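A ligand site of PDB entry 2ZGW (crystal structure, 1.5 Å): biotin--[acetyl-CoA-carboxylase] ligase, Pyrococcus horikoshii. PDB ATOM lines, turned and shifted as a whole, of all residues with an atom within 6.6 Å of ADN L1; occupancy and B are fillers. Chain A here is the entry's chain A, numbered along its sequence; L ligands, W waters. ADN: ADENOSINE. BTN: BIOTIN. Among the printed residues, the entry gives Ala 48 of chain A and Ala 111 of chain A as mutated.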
ATOM      1  N   ALA A  48      29.788  -4.106 -12.601  1.00  0.00           N
ATOM      2  CA  ALA A  48      30.179  -4.990 -13.690  1.00  0.00           C
ATOM      3  C   ALA A  48      31.436  -4.467 -14.367  1.00  0.00           C
ATOM      4  O   ALA A  48      31.711  -3.263 -14.364  1.00  0.00           O
ATOM      5  CB  ALA A  48      29.047  -5.107 -14.697  1.00  0.00           C
ATOM      6  N   ASN A  50      34.629  -4.682 -13.595  1.00  0.00           N
ATOM      7  CA  ASN A  50      35.577  -4.067 -12.671  1.00  0.00           C
ATOM      8  C   ASN A  50      35.386  -2.596 -12.312  1.00  0.00           C
ATOM      9  O   ASN A  50      36.357  -1.892 -12.036  1.00  0.00           O
ATOM     10  CB  ASN A  50      37.002  -4.237 -13.216  1.00  0.00           C
ATOM     11  CG  ASN A  50      37.377  -5.688 -13.426  1.00  0.00           C
ATOM     12  OD1 ASN A  50      37.605  -6.126 -14.549  1.00  0.00           O
ATOM     13  ND2 ASN A  50      37.433  -6.449 -12.336  1.00  0.00           N
ATOM     14  N   ARG A  51      34.143  -2.127 -12.290  1.00  0.00           N
ATOM     15  CA  ARG A  51      33.884  -0.730 -11.954  1.00  0.00           C
ATOM     16  C   ARG A  51      33.679  -0.581 -10.444  1.00  0.00           C
ATOM     17  O   ARG A  51      33.379  -1.553  -9.753  1.00  0.00           O
ATOM     18  CB  ARG A  51      32.619  -0.216 -12.635  1.00  0.00           C
ATOM     19  CG  ARG A  51      31.380  -0.980 -12.187  1.00  0.00           C
ATOM     20  CD  ARG A  51      30.189  -0.064 -11.974  1.00  0.00           C
ATOM     21  NE  ARG A  51      29.590   0.378 -13.224  1.00  0.00           N
ATOM     22  CZ  ARG A  51      28.303   0.651 -13.394  1.00  0.00           C
ATOM     23  NH1 ARG A  51      27.452   0.535 -12.390  1.00  0.00           N
ATOM     24  NH2 ARG A  51      27.872   1.037 -14.586  1.00  0.00           N
ATOM     25  N   LYS A  52      33.810   0.652  -9.957  1.00  0.00           N
ATOM     26  CA  LYS A  52      33.589   0.909  -8.538  1.00  0.00           C
ATOM     27  C   LYS A  52      32.155   1.346  -8.328  1.00  0.00           C
ATOM     28  O   LYS A  52      31.630   2.179  -9.072  1.00  0.00           O
ATOM     29  CB  LYS A  52      34.524   2.012  -8.031  1.00  0.00           C
ATOM     30  CG  LYS A  52      34.263   2.348  -6.566  1.00  0.00           C
ATOM     31  CD  LYS A  52      35.242   3.372  -6.019  1.00  0.00           C
ATOM     32  CE  LYS A  52      35.000   3.584  -4.533  1.00  0.00           C
ATOM     33  NZ  LYS A  52      35.102   2.304  -3.773  1.00  0.00           N
ATOM     34  N   TRP A  53      31.499   0.772  -7.322  1.00  0.00           N
ATOM     35  CA  TRP A  53      30.122   1.122  -7.025  1.00  0.00           C
ATOM     36  C   TRP A  53      30.078   1.816  -5.664  1.00  0.00           C
ATOM     37  O   TRP A  53      30.353   1.205  -4.634  1.00  0.00           O
ATOM     38  CB  TRP A  53      29.250  -0.136  -7.017  1.00  0.00           C
ATOM     39  CG  TRP A  53      27.811   0.147  -6.743  1.00  0.00           C
ATOM     40  CD1 TRP A  53      27.194   0.128  -5.519  1.00  0.00           C
ATOM     41  CD2 TRP A  53      26.806   0.543  -7.690  1.00  0.00           C
ATOM     42  NE1 TRP A  53      25.869   0.479  -5.652  1.00  0.00           N
ATOM     43  CE2 TRP A  53      25.604   0.730  -6.972  1.00  0.00           C
ATOM     44  CE3 TRP A  53      26.803   0.741  -9.076  1.00  0.00           C
ATOM     45  CZ2 TRP A  53      24.410   1.122  -7.598  1.00  0.00           C
ATOM     46  CZ3 TRP A  53      25.625   1.122  -9.695  1.00  0.00           C
ATOM     47  CH2 TRP A  53      24.439   1.311  -8.953  1.00  0.00           C
ATOM     48  N   GLU A  54      29.733   3.104  -5.676  1.00  0.00           N
ATOM     49  CA  GLU A  54      29.656   3.892  -4.450  1.00  0.00           C
ATOM     50  C   GLU A  54      28.526   3.332  -3.584  1.00  0.00           C
ATOM     51  O   GLU A  54      27.384   3.237  -4.037  1.00  0.00           O
ATOM     52  CB  GLU A  54      29.387   5.364  -4.767  1.00  0.00           C
ATOM     53  CG  GLU A  54      30.429   6.023  -5.658  1.00  0.00           C
ATOM     54  CD  GLU A  54      31.839   5.918  -5.100  1.00  0.00           C
ATOM     55  OE1 GLU A  54      32.024   6.235  -3.903  1.00  0.00           O
ATOM     56  OE2 GLU A  54      32.749   5.533  -5.852  1.00  0.00           O
ATOM     57  N   SER A  55      28.855   2.995  -2.344  1.00  0.00           N
ATOM     58  CA  SER A  55      27.887   2.395  -1.437  1.00  0.00           C
ATOM     59  C   SER A  55      27.838   3.056  -0.060  1.00  0.00           C
ATOM     60  O   SER A  55      28.109   2.411   0.956  1.00  0.00           O
ATOM     61  CB  SER A  55      28.205   0.909  -1.262  1.00  0.00           C
ATOM     62  OG  SER A  55      28.441   0.289  -2.524  1.00  0.00           O
ATOM     63  N   PRO A  56      27.486   4.340   0.002  1.00  0.00           N
ATOM     64  CA  PRO A  56      27.408   5.031   1.280  1.00  0.00           C
ATOM     65  C   PRO A  56      26.158   4.677   2.070  1.00  0.00           C
ATOM     66  O   PRO A  56      25.235   4.044   1.549  1.00  0.00           O
ATOM     67  CB  PRO A  56      27.439   6.497   0.886  1.00  0.00           C
ATOM     68  CG  PRO A  56      26.687   6.495  -0.403  1.00  0.00           C
ATOM     69  CD  PRO A  56      27.211   5.268  -1.119  1.00  0.00           C
ATOM     70  N   TRP A  61      22.242  -2.135  -0.196  1.00  0.00           N
ATOM     71  CA  TRP A  61      23.332  -2.903  -0.785  1.00  0.00           C
ATOM     72  C   TRP A  61      23.193  -4.351  -0.318  1.00  0.00           C
ATOM     73  O   TRP A  61      23.433  -4.650   0.858  1.00  0.00           O
ATOM     74  CB  TRP A  61      24.688  -2.333  -0.325  1.00  0.00           C
ATOM     75  CG  TRP A  61      24.712  -0.824  -0.201  1.00  0.00           C
ATOM     76  CD1 TRP A  61      25.032  -0.101   0.923  1.00  0.00           C
ATOM     77  CD2 TRP A  61      24.391   0.138  -1.214  1.00  0.00           C
ATOM     78  NE1 TRP A  61      24.931   1.241   0.668  1.00  0.00           N
ATOM     79  CE2 TRP A  61      24.538   1.412  -0.637  1.00  0.00           C
ATOM     80  CE3 TRP A  61      23.986   0.035  -2.548  1.00  0.00           C
ATOM     81  CZ2 TRP A  61      24.301   2.594  -1.358  1.00  0.00           C
ATOM     82  CZ3 TRP A  61      23.749   1.217  -3.269  1.00  0.00           C
ATOM     83  CH2 TRP A  61      23.914   2.478  -2.663  1.00  0.00           C
ATOM     84  N   ALA A 111      20.807   6.626 -13.454  1.00  0.00           N
ATOM     85  CA  ALA A 111      20.954   5.361 -12.749  1.00  0.00           C
ATOM     86  C   ALA A 111      20.531   5.394 -11.283  1.00  0.00           C
ATOM     87  O   ALA A 111      21.044   6.192 -10.494  1.00  0.00           O
ATOM     88  CB  ALA A 111      22.389   4.877 -12.854  1.00  0.00           C
ATOM     89  N   ILE A 112      19.594   4.524 -10.932  1.00  0.00           N
ATOM     90  CA  ILE A 112      19.113   4.437  -9.561  1.00  0.00           C
ATOM     91  C   ILE A 112      19.489   3.092  -8.948  1.00  0.00           C
ATOM     92  O   ILE A 112      19.499   2.934  -7.726  1.00  0.00           O
ATOM     93  CB  ILE A 112      17.566   4.631  -9.488  1.00  0.00           C
ATOM     94  CG1 ILE A 112      17.150   4.929  -8.056  1.00  0.00           C
ATOM     95  CG2 ILE A 112      16.856   3.380 -10.009  1.00  0.00           C
ATOM     96  CD1 ILE A 112      15.708   5.419  -7.923  1.00  0.00           C
ATOM     97  N   ALA A 113      19.828   2.116  -9.788  1.00  0.00           N
ATOM     98  CA  ALA A 113      20.199   0.796  -9.307  1.00  0.00           C
ATOM     99  C   ALA A 113      21.036   0.026 -10.313  1.00  0.00           C
ATOM    100  O   ALA A 113      20.983   0.277 -11.524  1.00  0.00           O
ATOM    101  CB  ALA A 113      18.945   0.004  -8.963  1.00  0.00           C
ATOM    102  N   GLY A 114      21.805  -0.925  -9.796  1.00  0.00           N
ATOM    103  CA  GLY A 114      22.658  -1.751 -10.626  1.00  0.00           C
ATOM    104  C   GLY A 114      22.628  -3.177 -10.103  1.00  0.00           C
ATOM    105  O   GLY A 114      22.532  -3.396  -8.886  1.00  0.00           O
ATOM    106  N   GLY A 129      22.327  -3.172  -5.987  1.00  0.00           N
ATOM    107  CA  GLY A 129      22.620  -1.926  -5.311  1.00  0.00           C
ATOM    108  C   GLY A 129      21.551  -0.931  -5.717  1.00  0.00           C
ATOM    109  O   GLY A 129      21.374  -0.664  -6.911  1.00  0.00           O
ATOM    110  N   LEU A 130      20.808  -0.400  -4.751  1.00  0.00           N
ATOM    111  CA  LEU A 130      19.738   0.551  -5.042  1.00  0.00           C
ATOM    112  C   LEU A 130      19.896   1.811  -4.205  1.00  0.00           C
ATOM    113  O   LEU A 130      19.940   1.739  -2.982  1.00  0.00           O
ATOM    114  CB  LEU A 130      18.384  -0.098  -4.744  1.00  0.00           C
ATOM    115  CG  LEU A 130      17.131   0.782  -4.720  1.00  0.00           C
ATOM    116  CD1 LEU A 130      16.876   1.357  -6.107  1.00  0.00           C
ATOM    117  CD2 LEU A 130      15.950  -0.058  -4.261  1.00  0.00           C
ATOM    118  N   ASN A 131      19.959   2.964  -4.861  1.00  0.00           N
ATOM    119  CA  ASN A 131      20.104   4.231  -4.134  1.00  0.00           C
ATOM    120  C   ASN A 131      18.765   4.611  -3.538  1.00  0.00           C
ATOM    121  O   ASN A 131      17.786   4.774  -4.257  1.00  0.00           O
ATOM    122  CB  ASN A 131      20.579   5.342  -5.073  1.00  0.00           C
ATOM    123  CG  ASN A 131      21.903   5.032  -5.731  1.00  0.00           C
ATOM    124  OD1 ASN A 131      22.858   4.640  -5.063  1.00  0.00           O
ATOM    125  ND2 ASN A 131      21.980   5.225  -7.042  1.00  0.00           N
ATOM    126  N   ASN A 134      20.805   7.702   0.186  1.00  0.00           N
ATOM    127  CA  ASN A 134      22.206   8.066   0.101  1.00  0.00           C
ATOM    128  C   ASN A 134      22.525   9.125  -0.953  1.00  0.00           C
ATOM    129  O   ASN A 134      21.744   9.361  -1.868  1.00  0.00           O
ATOM    130  CB  ASN A 134      23.047   6.832  -0.211  1.00  0.00           C
ATOM    131  CG  ASN A 134      22.565   6.098  -1.460  1.00  0.00           C
ATOM    132  OD1 ASN A 134      21.471   5.526  -1.470  1.00  0.00           O
ATOM    133  ND2 ASN A 134      23.373   6.121  -2.518  1.00  0.00           N
ATOM    134  N   LYS A 135      23.694   9.745  -0.796  1.00  0.00           N
ATOM    135  CA  LYS A 135      24.161  10.713  -1.770  1.00  0.00           C
ATOM    136  C   LYS A 135      24.597   9.831  -2.932  1.00  0.00           C
ATOM    137  O   LYS A 135      25.015   8.692  -2.722  1.00  0.00           O
ATOM    138  CB  LYS A 135      25.370  11.487  -1.234  1.00  0.00           C
ATOM    139  CG  LYS A 135      25.064  12.363  -0.025  1.00  0.00           C
ATOM    140  CD  LYS A 135      26.327  13.085   0.452  1.00  0.00           C
ATOM    141  CE  LYS A 135      26.084  13.833   1.758  1.00  0.00           C
ATOM    142  NZ  LYS A 135      25.084  14.934   1.612  1.00  0.00           N
ATOM    143  N   VAL A 136      24.497  10.336  -4.158  1.00  0.00           N
ATOM    144  CA  VAL A 136      24.864   9.553  -5.328  1.00  0.00           C
ATOM    145  C   VAL A 136      25.840  10.295  -6.233  1.00  0.00           C
ATOM    146  O   VAL A 136      26.006  11.506  -6.112  1.00  0.00           O
ATOM    147  CB  VAL A 136      23.611   9.182  -6.164  1.00  0.00           C
ATOM    148  CG1 VAL A 136      22.647   8.369  -5.314  1.00  0.00           C
ATOM    149  CG2 VAL A 136      22.929  10.440  -6.682  1.00  0.00           C
ATOM    150  N   PRO A 137      26.500   9.567  -7.146  1.00  0.00           N
ATOM    151  CA  PRO A 137      27.444  10.197  -8.067  1.00  0.00           C
ATOM    152  C   PRO A 137      26.689  11.190  -8.949  1.00  0.00           C
ATOM    153  O   PRO A 137      25.481  11.038  -9.154  1.00  0.00           O
ATOM    154  CB  PRO A 137      27.984   9.029  -8.876  1.00  0.00           C
ATOM    155  CG  PRO A 137      27.879   7.876  -7.935  1.00  0.00           C
ATOM    156  CD  PRO A 137      26.537   8.100  -7.284  1.00  0.00           C
ATOM    157  N   ASN A 138      27.389  12.187  -9.476  1.00  0.00           N
ATOM    158  CA  ASN A 138      26.762  13.163 -10.352  1.00  0.00           C
ATOM    159  C   ASN A 138      26.134  12.389 -11.504  1.00  0.00           C
ATOM    160  O   ASN A 138      26.759  11.487 -12.072  1.00  0.00           O
ATOM    161  CB  ASN A 138      27.802  14.152 -10.902  1.00  0.00           C
ATOM    162  CG  ASN A 138      28.429  15.023  -9.834  1.00  0.00           C
ATOM    163  OD1 ASN A 138      28.091  14.914  -8.653  1.00  0.00           O
ATOM    164  ND2 ASN A 138      29.354  15.901 -10.232  1.00  0.00           N
ATOM    165  N   GLY A 139      24.898  12.720 -11.853  1.00  0.00           N
ATOM    166  CA  GLY A 139      24.248  12.024 -12.944  1.00  0.00           C
ATOM    167  C   GLY A 139      23.348  10.870 -12.543  1.00  0.00           C
ATOM    168  O   GLY A 139      22.479  10.450 -13.297  1.00  0.00           O
ATOM    169  N   ALA A 140      23.575  10.323 -11.348  1.00  0.00           N
ATOM    170  CA  ALA A 140      22.750   9.216 -10.863  1.00  0.00           C
ATOM    171  C   ALA A 140      21.579   9.813 -10.089  1.00  0.00           C
ATOM    172  O   ALA A 140      21.448  11.026  -9.996  1.00  0.00           O
ATOM    173  CB  ALA A 140      23.572   8.311  -9.961  1.00  0.00           C
ATOM    174  N   THR A 141      20.729   8.959  -9.550  1.00  0.00           N
ATOM    175  CA  THR A 141      19.595   9.444  -8.773  1.00  0.00           C
ATOM    176  C   THR A 141      19.255   8.449  -7.686  1.00  0.00           C
ATOM    177  O   THR A 141      19.871   7.375  -7.595  1.00  0.00           O
ATOM    178  CB  THR A 141      18.361   9.721  -9.680  1.00  0.00           C
ATOM    179  OG1 THR A 141      17.373  10.432  -8.935  1.00  0.00           O
ATOM    180  CG2 THR A 141      17.758   8.418 -10.204  1.00  0.00           C
HETATM  181  O5' ADN L   1      32.132   2.600 -13.048  1.00  0.00           O
HETATM  182  C5' ADN L   1      31.717   3.946 -12.795  1.00  0.00           C
HETATM  183  C4' ADN L   1      30.208   4.081 -13.036  1.00  0.00           C
HETATM  184  O4' ADN L   1      29.451   3.470 -11.943  1.00  0.00           O
HETATM  185  C3' ADN L   1      29.799   5.548 -13.146  1.00  0.00           C
HETATM  186  O3' ADN L   1      29.051   5.816 -14.334  1.00  0.00           O
HETATM  187  C2' ADN L   1      29.010   5.801 -11.857  1.00  0.00           C
HETATM  188  O2' ADN L   1      28.000   6.823 -11.989  1.00  0.00           O
HETATM  189  C1' ADN L   1      28.415   4.414 -11.557  1.00  0.00           C
HETATM  190  N9  ADN L   1      28.081   4.347 -10.130  1.00  0.00           N
HETATM  191  C8  ADN L   1      28.920   4.047  -9.090  1.00  0.00           C
HETATM  192  N7  ADN L   1      28.116   4.038  -7.865  1.00  0.00           N
HETATM  193  C5  ADN L   1      26.845   4.321  -8.181  1.00  0.00           C
HETATM  194  C6  ADN L   1      25.621   4.450  -7.478  1.00  0.00           C
HETATM  195  N6  ADN L   1      25.568   4.254  -6.107  1.00  0.00           N
HETATM  196  N1  ADN L   1      24.465   4.739  -8.177  1.00  0.00           N
HETATM  197  C2  ADN L   1      24.455   4.919  -9.519  1.00  0.00           C
HETATM  198  N3  ADN L   1      25.589   4.805 -10.228  1.00  0.00           N
HETATM  199  C4  ADN L   1      26.794   4.527  -9.624  1.00  0.00           C
HETATM  200  C11 BTN L   2      26.529  -2.409 -12.030  1.00  0.00           C
HETATM  201  O11 BTN L   2      25.726  -1.473 -12.215  1.00  0.00           O
HETATM  202  O12 BTN L   2      27.557  -2.558 -12.760  1.00  0.00           O
HETATM  203  C10 BTN L   2      26.313  -3.417 -10.950  1.00  0.00           C
HETATM  204  C9  BTN L   2      26.339  -2.846  -9.565  1.00  0.00           C
HETATM  205  C8  BTN L   2      26.047  -3.862  -8.503  1.00  0.00           C
HETATM  206  C7  BTN L   2      26.076  -3.244  -7.106  1.00  0.00           C
HETATM  207  C2  BTN L   2      25.780  -4.194  -5.954  1.00  0.00           C
HETATM  208  S1  BTN L   2      25.827  -3.411  -4.355  1.00  0.00           S
HETATM  209  C6  BTN L   2      25.471  -5.029  -3.624  1.00  0.00           C
HETATM  210  C5  BTN L   2      26.532  -5.915  -4.343  1.00  0.00           C
HETATM  211  N1  BTN L   2      27.869  -5.843  -3.717  1.00  0.00           N
HETATM  212  C3  BTN L   2      28.766  -5.376  -4.615  1.00  0.00           C
HETATM  213  O3  BTN L   2      29.987  -5.196  -4.391  1.00  0.00           O
HETATM  214  N2  BTN L   2      28.160  -5.124  -5.825  1.00  0.00           N
HETATM  215  C4  BTN L   2      26.743  -5.428  -5.789  1.00  0.00           C
HETATM  216  O   HOH W   1      30.993   4.477 -16.836  1.00  0.00           O
HETATM  217  O   HOH W   2      28.539   6.482 -16.836  1.00  0.00           O
HETATM  218  O   HOH W   3      25.393   3.202 -12.936  1.00  0.00           O
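Residues that only touch ADN L1: Lys 52 (3.3 Å), Trp 53 (3.5 Å), Ala 140 (3.5 Å), Pro 137 (3.7 Å) and Ala 111 (3.8 Å). Hydrophobic or aromatic side chains that line ADN L1: Trp 53, Ala 111, Pro 137 and Ala 140. Of the 24 residues printed, 8 come within 4 Å of ADN L1.
O of Thr 141 is in hydrogen-bond range of ND2 of Asn 131, 3.1 Å away. OD1 of Asn 131 sits at hydrogen-bond distance from ND2 of Asn 134, 3.0 Å away. O of Trp 53 sits at hydrogen-bond distance from OG of Ser 55, at 3.0 Å. The backbone carbonyl oxygen (O) of Ala 111 is in hydrogen-bond range of the backbone NH (N) of Thr 141. The backbone NH (N) of Asn 131 sits at hydrogen-bond distance from the backbone carbonyl oxygen (O) of Ile 112 (2.9 Å).
Water W3 lies within hydrogen-bond range of N3 of ADN L1 (3.2 Å) and NH1 of Arg 51 (3.4 Å).
N7 of ADN L1 sits at hydrogen-bond distance from N of Glu 54. The guanidinium group (NH1) of Arg 51 is in salt-bridge range of an oxygen (O11) of BTN L2 (2.7 Å). N1 of ADN L1 lies within hydrogen-bond range of ND2 of Asn 131. O of Glu 54 sits at hydrogen-bond distance from N6 of ADN L1, 2.9 Å away. An oxygen (O4') of ADN L1 is in hydrogen-bond range of the guanidinium group (NE) of Arg 51 (3.3 Å). An oxygen (O12) of BTN L2 sits at hydrogen-bond distance from the backbone NH of Ala 48, at 2.7 Å.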
